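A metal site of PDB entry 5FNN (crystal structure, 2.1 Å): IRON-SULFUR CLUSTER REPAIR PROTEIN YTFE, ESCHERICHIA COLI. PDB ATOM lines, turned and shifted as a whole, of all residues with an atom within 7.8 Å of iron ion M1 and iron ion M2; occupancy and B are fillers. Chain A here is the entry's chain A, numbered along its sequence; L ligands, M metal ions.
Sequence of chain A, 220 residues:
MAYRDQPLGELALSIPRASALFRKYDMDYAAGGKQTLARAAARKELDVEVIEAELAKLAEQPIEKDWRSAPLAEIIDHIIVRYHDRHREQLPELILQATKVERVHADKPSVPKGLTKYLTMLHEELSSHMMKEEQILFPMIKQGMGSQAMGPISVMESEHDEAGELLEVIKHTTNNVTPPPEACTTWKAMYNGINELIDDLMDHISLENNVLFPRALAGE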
ATOM      1  N   ILE A  79       2.064  16.800 -28.542  1.00  0.00           N
ATOM      2  CA  ILE A  79       1.339  15.984 -27.580  1.00  0.00           C
ATOM      3  C   ILE A  79       2.181  14.803 -27.125  1.00  0.00           C
ATOM      4  O   ILE A  79       2.285  14.533 -25.924  1.00  0.00           O
ATOM      5  CB  ILE A  79       0.004  15.485 -28.140  1.00  0.00           C
ATOM      6  CG1 ILE A  79      -0.991  16.639 -28.238  1.00  0.00           C
ATOM      7  CG2 ILE A  79      -0.555  14.367 -27.264  1.00  0.00           C
ATOM      8  CD1 ILE A  79      -2.231  16.324 -29.035  1.00  0.00           C
ATOM      9  N   ILE A  80       2.785  14.091 -28.071  1.00  0.00           N
ATOM     10  CA  ILE A  80       3.591  12.898 -27.736  1.00  0.00           C
ATOM     11  C   ILE A  80       4.723  13.249 -26.782  1.00  0.00           C
ATOM     12  O   ILE A  80       4.941  12.540 -25.801  1.00  0.00           O
ATOM     13  CB  ILE A  80       4.143  12.206 -28.979  1.00  0.00           C
ATOM     14  CG1 ILE A  80       3.020  11.524 -29.754  1.00  0.00           C
ATOM     15  CG2 ILE A  80       5.182  11.157 -28.623  1.00  0.00           C
ATOM     16  CD1 ILE A  80       3.397  11.156 -31.195  1.00  0.00           C
ATOM     17  N   TYR A  83       3.324  15.920 -23.502  1.00  0.00           N
ATOM     18  CA  TYR A  83       2.348  15.281 -22.617  1.00  0.00           C
ATOM     19  C   TYR A  83       2.530  13.772 -22.430  1.00  0.00           C
ATOM     20  O   TYR A  83       2.755  13.337 -21.307  1.00  0.00           O
ATOM     21  CB  TYR A  83       0.926  15.648 -23.068  1.00  0.00           C
ATOM     22  CG  TYR A  83       0.694  17.139 -22.969  1.00  0.00           C
ATOM     23  CD1 TYR A  83       0.832  17.813 -21.762  1.00  0.00           C
ATOM     24  CD2 TYR A  83       0.347  17.888 -24.077  1.00  0.00           C
ATOM     25  CE1 TYR A  83       0.627  19.183 -21.655  1.00  0.00           C
ATOM     26  CE2 TYR A  83       0.138  19.265 -23.982  1.00  0.00           C
ATOM     27  CZ  TYR A  83       0.285  19.900 -22.769  1.00  0.00           C
ATOM     28  OH  TYR A  83       0.049  21.245 -22.649  1.00  0.00           O
ATOM     29  N   HIS A  84       2.468  12.965 -23.497  1.00  0.00           N
ATOM     30  CA  HIS A  84       2.507  11.499 -23.287  1.00  0.00           C
ATOM     31  C   HIS A  84       3.771  11.034 -22.580  1.00  0.00           C
ATOM     32  O   HIS A  84       3.698  10.304 -21.587  1.00  0.00           O
ATOM     33  CB  HIS A  84       2.374  10.691 -24.576  1.00  0.00           C
ATOM     34  CG  HIS A  84       1.039  10.768 -25.219  1.00  0.00           C
ATOM     35  ND1 HIS A  84       0.700   9.975 -26.308  1.00  0.00           N
ATOM     36  CD2 HIS A  84      -0.037  11.547 -24.970  1.00  0.00           C
ATOM     37  CE1 HIS A  84      -0.551  10.217 -26.651  1.00  0.00           C
ATOM     38  NE2 HIS A  84      -1.013  11.182 -25.871  1.00  0.00           N
ATOM     39  N   HIS A  87       3.774  12.106 -18.935  1.00  0.00           N
ATOM     40  CA  HIS A  87       2.892  11.298 -18.065  1.00  0.00           C
ATOM     41  C   HIS A  87       3.539   9.950 -17.769  1.00  0.00           C
ATOM     42  O   HIS A  87       3.456   9.457 -16.668  1.00  0.00           O
ATOM     43  CB  HIS A  87       1.522  11.044 -18.690  1.00  0.00           C
ATOM     44  CG  HIS A  87       0.751  12.276 -19.031  1.00  0.00           C
ATOM     45  ND1 HIS A  87       0.822  13.427 -18.286  1.00  0.00           N
ATOM     46  CD2 HIS A  87      -0.190  12.510 -19.977  1.00  0.00           C
ATOM     47  CE1 HIS A  87      -0.019  14.331 -18.772  1.00  0.00           C
ATOM     48  NE2 HIS A  87      -0.641  13.798 -19.809  1.00  0.00           N
ATOM     49  N   LEU A 126      -4.237   5.220 -18.807  1.00  0.00           N
ATOM     50  CA  LEU A 126      -3.557   6.163 -19.677  1.00  0.00           C
ATOM     51  C   LEU A 126      -2.573   5.476 -20.606  1.00  0.00           C
ATOM     52  O   LEU A 126      -2.449   5.853 -21.791  1.00  0.00           O
ATOM     53  CB  LEU A 126      -2.757   7.202 -18.894  1.00  0.00           C
ATOM     54  CG  LEU A 126      -3.199   8.629 -18.736  1.00  0.00           C
ATOM     55  CD1 LEU A 126      -2.040   9.442 -18.120  1.00  0.00           C
ATOM     56  CD2 LEU A 126      -3.657   9.237 -20.037  1.00  0.00           C
ATOM     57  N   HIS A 129      -4.393   3.717 -23.402  1.00  0.00           N
ATOM     58  CA  HIS A 129      -5.032   4.785 -24.173  1.00  0.00           C
ATOM     59  C   HIS A 129      -4.011   5.490 -25.068  1.00  0.00           C
ATOM     60  O   HIS A 129      -4.227   5.600 -26.287  1.00  0.00           O
ATOM     61  CB  HIS A 129      -5.726   5.746 -23.222  1.00  0.00           C
ATOM     62  CG  HIS A 129      -6.210   7.014 -23.860  1.00  0.00           C
ATOM     63  ND1 HIS A 129      -7.502   7.185 -24.323  1.00  0.00           N
ATOM     64  CD2 HIS A 129      -5.582   8.198 -24.057  1.00  0.00           C
ATOM     65  CE1 HIS A 129      -7.637   8.405 -24.791  1.00  0.00           C
ATOM     66  NE2 HIS A 129      -6.494   9.054 -24.627  1.00  0.00           N
ATOM     67  N   MET A 130      -2.905   5.932 -24.491  1.00  0.00           N
ATOM     68  CA  MET A 130      -1.849   6.630 -25.243  1.00  0.00           C
ATOM     69  C   MET A 130      -1.208   5.782 -26.322  1.00  0.00           C
ATOM     70  O   MET A 130      -0.857   6.303 -27.385  1.00  0.00           O
ATOM     71  CB  MET A 130      -0.758   7.126 -24.320  1.00  0.00           C
ATOM     72  CG  MET A 130      -1.277   8.305 -23.491  1.00  0.00           C
ATOM     73  SD  MET A 130       0.153   8.990 -22.290  1.00  0.00           S
ATOM     74  CE  MET A 130       0.766   7.342 -21.376  1.00  0.00           C
ATOM     75  N   MET A 131      -1.081   4.480 -26.075  1.00  0.00           N
ATOM     76  CA  MET A 131      -0.516   3.548 -27.071  1.00  0.00           C
ATOM     77  C   MET A 131      -1.389   3.450 -28.282  1.00  0.00           C
ATOM     78  O   MET A 131      -0.880   3.443 -29.411  1.00  0.00           O
ATOM     79  CB  MET A 131      -0.345   2.135 -26.494  1.00  0.00           C
ATOM     80  CG  MET A 131       0.104   1.072 -27.522  1.00  0.00           C
ATOM     81  SD  MET A 131       0.337  -0.670 -26.626  1.00  0.00           S
ATOM     82  CE  MET A 131       1.970  -0.232 -25.581  1.00  0.00           C
ATOM     83  N   GLU A 133      -3.502   5.828 -29.286  1.00  0.00           N
ATOM     84  CA  GLU A 133      -3.359   7.110 -29.985  1.00  0.00           C
ATOM     85  C   GLU A 133      -2.087   7.093 -30.816  1.00  0.00           C
ATOM     86  O   GLU A 133      -2.110   7.454 -31.989  1.00  0.00           O
ATOM     87  CB  GLU A 133      -3.388   8.331 -29.028  1.00  0.00           C
ATOM     88  CG  GLU A 133      -4.741   8.531 -28.374  1.00  0.00           C
ATOM     89  CD  GLU A 133      -4.868   9.780 -27.503  1.00  0.00           C
ATOM     90  OE1 GLU A 133      -3.842  10.231 -26.887  1.00  0.00           O
ATOM     91  OE2 GLU A 133      -6.041  10.285 -27.398  1.00  0.00           O
ATOM     92  N   GLU A 134      -0.987   6.652 -30.223  1.00  0.00           N
ATOM     93  CA  GLU A 134       0.307   6.701 -30.903  1.00  0.00           C
ATOM     94  C   GLU A 134       0.452   5.693 -32.051  1.00  0.00           C
ATOM     95  O   GLU A 134       1.157   5.988 -33.030  1.00  0.00           O
ATOM     96  CB  GLU A 134       1.458   6.523 -29.923  1.00  0.00           C
ATOM     97  CG  GLU A 134       1.748   7.781 -29.122  1.00  0.00           C
ATOM     98  CD  GLU A 134       2.760   7.584 -28.020  1.00  0.00           C
ATOM     99  OE1 GLU A 134       3.612   6.686 -28.151  1.00  0.00           O
ATOM    100  OE2 GLU A 134       2.701   8.310 -27.013  1.00  0.00           O
ATOM    101  N   LEU A 137      -4.386   6.206 -34.112  1.00  0.00           N
ATOM    102  CA  LEU A 137      -5.103   7.454 -34.384  1.00  0.00           C
ATOM    103  C   LEU A 137      -4.228   8.593 -34.897  1.00  0.00           C
ATOM    104  O   LEU A 137      -4.589   9.277 -35.855  1.00  0.00           O
ATOM    105  CB  LEU A 137      -5.878   7.937 -33.173  1.00  0.00           C
ATOM    106  CG  LEU A 137      -6.605   9.266 -33.315  1.00  0.00           C
ATOM    107  CD1 LEU A 137      -7.621   9.220 -34.444  1.00  0.00           C
ATOM    108  CD2 LEU A 137      -7.317   9.612 -32.024  1.00  0.00           C
ATOM    109  N   PHE A 138      -3.095   8.811 -34.237  1.00  0.00           N
ATOM    110  CA  PHE A 138      -2.148   9.841 -34.664  1.00  0.00           C
ATOM    111  C   PHE A 138      -1.565   9.579 -36.089  1.00  0.00           C
ATOM    112  O   PHE A 138      -1.645  10.479 -36.935  1.00  0.00           O
ATOM    113  CB  PHE A 138      -1.065  10.058 -33.600  1.00  0.00           C
ATOM    114  CG  PHE A 138      -1.567  10.725 -32.313  1.00  0.00           C
ATOM    115  CD1 PHE A 138      -2.857  11.263 -32.193  1.00  0.00           C
ATOM    116  CD2 PHE A 138      -0.712  10.862 -31.239  1.00  0.00           C
ATOM    117  CE1 PHE A 138      -3.273  11.854 -31.026  1.00  0.00           C
ATOM    118  CE2 PHE A 138      -1.116  11.491 -30.088  1.00  0.00           C
ATOM    119  CZ  PHE A 138      -2.401  11.975 -29.970  1.00  0.00           C
ATOM    120  N   MET A 156     -11.793   7.456 -27.863  1.00  0.00           N
ATOM    121  CA  MET A 156     -10.813   8.285 -27.139  1.00  0.00           C
ATOM    122  C   MET A 156     -11.499   9.291 -26.225  1.00  0.00           C
ATOM    123  O   MET A 156     -11.051   9.533 -25.106  1.00  0.00           O
ATOM    124  CB  MET A 156      -9.869   9.097 -28.040  1.00  0.00           C
ATOM    125  CG  MET A 156      -8.907   8.304 -28.923  1.00  0.00           C
ATOM    126  SD  MET A 156      -7.914   6.915 -27.943  1.00  0.00           S
ATOM    127  CE  MET A 156      -9.013   5.397 -28.558  1.00  0.00           C
ATOM    128  N   GLU A 157     -12.590   9.888 -26.708  1.00  0.00           N
ATOM    129  CA  GLU A 157     -13.342  10.879 -25.893  1.00  0.00           C
ATOM    130  C   GLU A 157     -14.051  10.262 -24.706  1.00  0.00           C
ATOM    131  O   GLU A 157     -14.056  10.847 -23.618  1.00  0.00           O
ATOM    132  CB  GLU A 157     -14.289  11.723 -26.744  1.00  0.00           C
ATOM    133  CG  GLU A 157     -13.528  12.728 -27.623  1.00  0.00           C
ATOM    134  CD  GLU A 157     -14.435  13.677 -28.429  1.00  0.00           C
ATOM    135  OE1 GLU A 157     -15.665  13.440 -28.490  1.00  0.00           O
ATOM    136  OE2 GLU A 157     -13.913  14.661 -29.012  1.00  0.00           O
ATOM    137  N   GLU A 159     -12.927   7.654 -23.147  1.00  0.00           N
ATOM    138  CA  GLU A 159     -11.780   7.408 -22.229  1.00  0.00           C
ATOM    139  C   GLU A 159     -11.244   8.650 -21.546  1.00  0.00           C
ATOM    140  O   GLU A 159     -10.913   8.594 -20.365  1.00  0.00           O
ATOM    141  CB  GLU A 159     -10.676   6.643 -22.954  1.00  0.00           C
ATOM    142  CG  GLU A 159     -11.136   5.212 -23.256  1.00  0.00           C
ATOM    143  CD  GLU A 159     -10.139   4.403 -24.056  1.00  0.00           C
ATOM    144  OE1 GLU A 159      -9.075   4.932 -24.451  1.00  0.00           O
ATOM    145  OE2 GLU A 159     -10.408   3.223 -24.313  1.00  0.00           O
ATOM    146  N   HIS A 160     -11.258   9.800 -22.226  1.00  0.00           N
ATOM    147  CA  HIS A 160     -10.941  11.073 -21.568  1.00  0.00           C
ATOM    148  C   HIS A 160     -11.889  11.402 -20.427  1.00  0.00           C
ATOM    149  O   HIS A 160     -11.429  11.919 -19.408  1.00  0.00           O
ATOM    150  CB  HIS A 160     -10.999  12.250 -22.535  1.00  0.00           C
ATOM    151  CG  HIS A 160      -9.931  12.214 -23.556  1.00  0.00           C
ATOM    152  ND1 HIS A 160      -9.943  13.007 -24.680  1.00  0.00           N
ATOM    153  CD2 HIS A 160      -8.838  11.420 -23.661  1.00  0.00           C
ATOM    154  CE1 HIS A 160      -8.898  12.716 -25.432  1.00  0.00           C
ATOM    155  NE2 HIS A 160      -8.213  11.758 -24.838  1.00  0.00           N
ATOM    156  N   LEU A 201      -2.506  16.985 -17.807  1.00  0.00           N
ATOM    157  CA  LEU A 201      -3.495  16.087 -18.359  1.00  0.00           C
ATOM    158  C   LEU A 201      -4.734  16.841 -18.885  1.00  0.00           C
ATOM    159  O   LEU A 201      -5.284  16.478 -19.926  1.00  0.00           O
ATOM    160  CB  LEU A 201      -3.827  15.004 -17.336  1.00  0.00           C
ATOM    161  CG  LEU A 201      -4.610  13.776 -17.760  1.00  0.00           C
ATOM    162  CD1 LEU A 201      -4.152  13.130 -19.060  1.00  0.00           C
ATOM    163  CD2 LEU A 201      -4.544  12.765 -16.615  1.00  0.00           C
ATOM    164  N   HIS A 204      -3.569  18.584 -22.090  1.00  0.00           N
ATOM    165  CA  HIS A 204      -3.447  17.468 -23.041  1.00  0.00           C
ATOM    166  C   HIS A 204      -4.835  17.101 -23.600  1.00  0.00           C
ATOM    167  O   HIS A 204      -5.055  17.153 -24.810  1.00  0.00           O
ATOM    168  CB  HIS A 204      -2.772  16.304 -22.286  1.00  0.00           C
ATOM    169  CG  HIS A 204      -2.708  15.017 -23.042  1.00  0.00           C
ATOM    170  ND1 HIS A 204      -2.417  13.816 -22.435  1.00  0.00           N
ATOM    171  CD2 HIS A 204      -2.954  14.727 -24.335  1.00  0.00           C
ATOM    172  CE1 HIS A 204      -2.465  12.848 -23.327  1.00  0.00           C
ATOM    173  NE2 HIS A 204      -2.793  13.374 -24.484  1.00  0.00           N
ATOM    174  N   ILE A 205      -5.781  16.784 -22.710  1.00  0.00           N
ATOM    175  CA  ILE A 205      -7.130  16.403 -23.115  1.00  0.00           C
ATOM    176  C   ILE A 205      -7.814  17.559 -23.899  1.00  0.00           C
ATOM    177  O   ILE A 205      -8.490  17.318 -24.907  1.00  0.00           O
ATOM    178  CB  ILE A 205      -8.036  15.979 -21.926  1.00  0.00           C
ATOM    179  CG1 ILE A 205      -7.566  14.706 -21.197  1.00  0.00           C
ATOM    180  CG2 ILE A 205      -9.501  15.809 -22.341  1.00  0.00           C
ATOM    181  CD1 ILE A 205      -6.912  13.682 -22.048  1.00  0.00           C
ATOM    182  N   GLU A 208      -6.555  17.764 -27.439  1.00  0.00           N
ATOM    183  CA  GLU A 208      -7.154  16.703 -28.219  1.00  0.00           C
ATOM    184  C   GLU A 208      -8.660  16.947 -28.512  1.00  0.00           C
ATOM    185  O   GLU A 208      -9.059  16.981 -29.690  1.00  0.00           O
ATOM    186  CB  GLU A 208      -6.898  15.328 -27.597  1.00  0.00           C
ATOM    187  CG  GLU A 208      -5.416  14.946 -27.698  1.00  0.00           C
ATOM    188  CD  GLU A 208      -5.035  13.644 -27.016  1.00  0.00           C
ATOM    189  OE1 GLU A 208      -5.890  12.975 -26.378  1.00  0.00           O
ATOM    190  OE2 GLU A 208      -3.818  13.334 -27.018  1.00  0.00           O
ATOM    191  N   ASN A 209      -9.447  17.185 -27.468  1.00  0.00           N
ATOM    192  CA  ASN A 209     -10.901  17.365 -27.610  1.00  0.00           C
ATOM    193  C   ASN A 209     -11.295  18.641 -28.349  1.00  0.00           C
ATOM    194  O   ASN A 209     -12.240  18.613 -29.137  1.00  0.00           O
ATOM    195  CB  ASN A 209     -11.603  17.342 -26.245  1.00  0.00           C
ATOM    196  CG  ASN A 209     -11.807  15.939 -25.692  1.00  0.00           C
ATOM    197  OD1 ASN A 209     -11.150  14.995 -26.080  1.00  0.00           O
ATOM    198  ND2 ASN A 209     -12.731  15.808 -24.767  1.00  0.00           N
ATOM    199  N   LEU A 212      -7.402  19.076 -31.963  1.00  0.00           N
ATOM    200  CA  LEU A 212      -6.967  17.994 -32.837  1.00  0.00           C
ATOM    201  C   LEU A 212      -8.113  17.182 -33.412  1.00  0.00           C
ATOM    202  O   LEU A 212      -8.175  16.984 -34.637  1.00  0.00           O
ATOM    203  CB  LEU A 212      -5.983  17.055 -32.154  1.00  0.00           C
ATOM    204  CG  LEU A 212      -5.454  15.899 -33.007  1.00  0.00           C
ATOM    205  CD1 LEU A 212      -4.651  16.417 -34.199  1.00  0.00           C
ATOM    206  CD2 LEU A 212      -4.583  14.982 -32.165  1.00  0.00           C
ATOM    207  N   PHE A 213      -9.000  16.699 -32.548  1.00  0.00           N
ATOM    208  CA  PHE A 213     -10.079  15.821 -32.952  1.00  0.00           C
ATOM    209  C   PHE A 213     -11.142  16.482 -33.879  1.00  0.00           C
ATOM    210  O   PHE A 213     -11.472  15.906 -34.899  1.00  0.00           O
ATOM    211  CB  PHE A 213     -10.747  15.149 -31.737  1.00  0.00           C
ATOM    212  CG  PHE A 213      -9.849  14.168 -30.967  1.00  0.00           C
ATOM    213  CD1 PHE A 213      -8.598  13.750 -31.438  1.00  0.00           C
ATOM    214  CD2 PHE A 213     -10.303  13.624 -29.770  1.00  0.00           C
ATOM    215  CE1 PHE A 213      -7.825  12.857 -30.712  1.00  0.00           C
ATOM    216  CE2 PHE A 213      -9.525  12.722 -29.042  1.00  0.00           C
ATOM    217  CZ  PHE A 213      -8.293  12.342 -29.508  1.00  0.00           C
HETATM  218  O1  LIG L   1      -4.577  11.152 -24.516  1.00  0.00           O
HETATM  219 FE    FE M   1      -3.237  11.788 -25.835  1.00  0.00          FE
HETATM  220 FE    FE M   2      -6.161  11.073 -25.521  1.00  0.00          FE
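A ring nitrogen (ND1) of His 204 lies within hydrogen-bond range of a ring nitrogen (NE2) of His 87, at 3.2 Å.
The side-chain carboxylate of Glu 134 sits at hydrogen-bond distance from a ring nitrogen (ND1) of His 84 (2.7 Å).
The backbone carbonyl oxygen of Glu 208 sits at hydrogen-bond distance from the backbone NH of Phe 213 (2.9 Å).
A ring nitrogen (ND1) of His 129 lies within hydrogen-bond range of the side-chain carboxylate of Glu 159.
ND1 of His 160 sits at hydrogen-bond distance from OD1 of Asn 209 (2.7 Å).
ND1 of His 129 sits close to SD of Met 156 (3.7 Å).
The backbone NH (N) of Phe 138 sits at hydrogen-bond distance from the backbone carbonyl oxygen (O) of Glu 133, at 2.8 Å.
The backbone NH of His 84 lies within hydrogen-bond range of the backbone carbonyl oxygen of Ile 79 (2.9 Å).
Ile 79 touches iron ion M1 (CG2 to FE, 3.99 Å).
Five residues have an atom within 4 Å of iron ion M1: Ile 79, His 84, Glu 133, His 204 and Glu 208.
The nearest printed residue that does not touch iron ion M1 is Phe 138 (4.2 Å).
Four residues have an atom within 4 Å of iron ion M2: His 129, Glu 133, His 160 and Glu 208.
Iron ion M1 is bound by the side-chain carboxylate (OE1) of Glu 133, an oxygen (O1) of the ligand, the side-chain carboxylate (OE2) of Glu 208, a ring nitrogen (NE2) of His 204 and a ring nitrogen (NE2) of His 84.
Iron ion M1 has five donor atoms within binding distance.
Iron ion M2 is bound by O1 of the ligand (1.9 Å), OE2 of Glu 133 (2.0 Å), OE1 of Glu 208 (2.1 Å), NE2 of His 129 (2.2 Å) and NE2 of His 160 (2.3 Å).
Slightly farther from iron ion M2 lies the side-chain carboxylate (OE1) of Glu 133 (2.8 Å).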
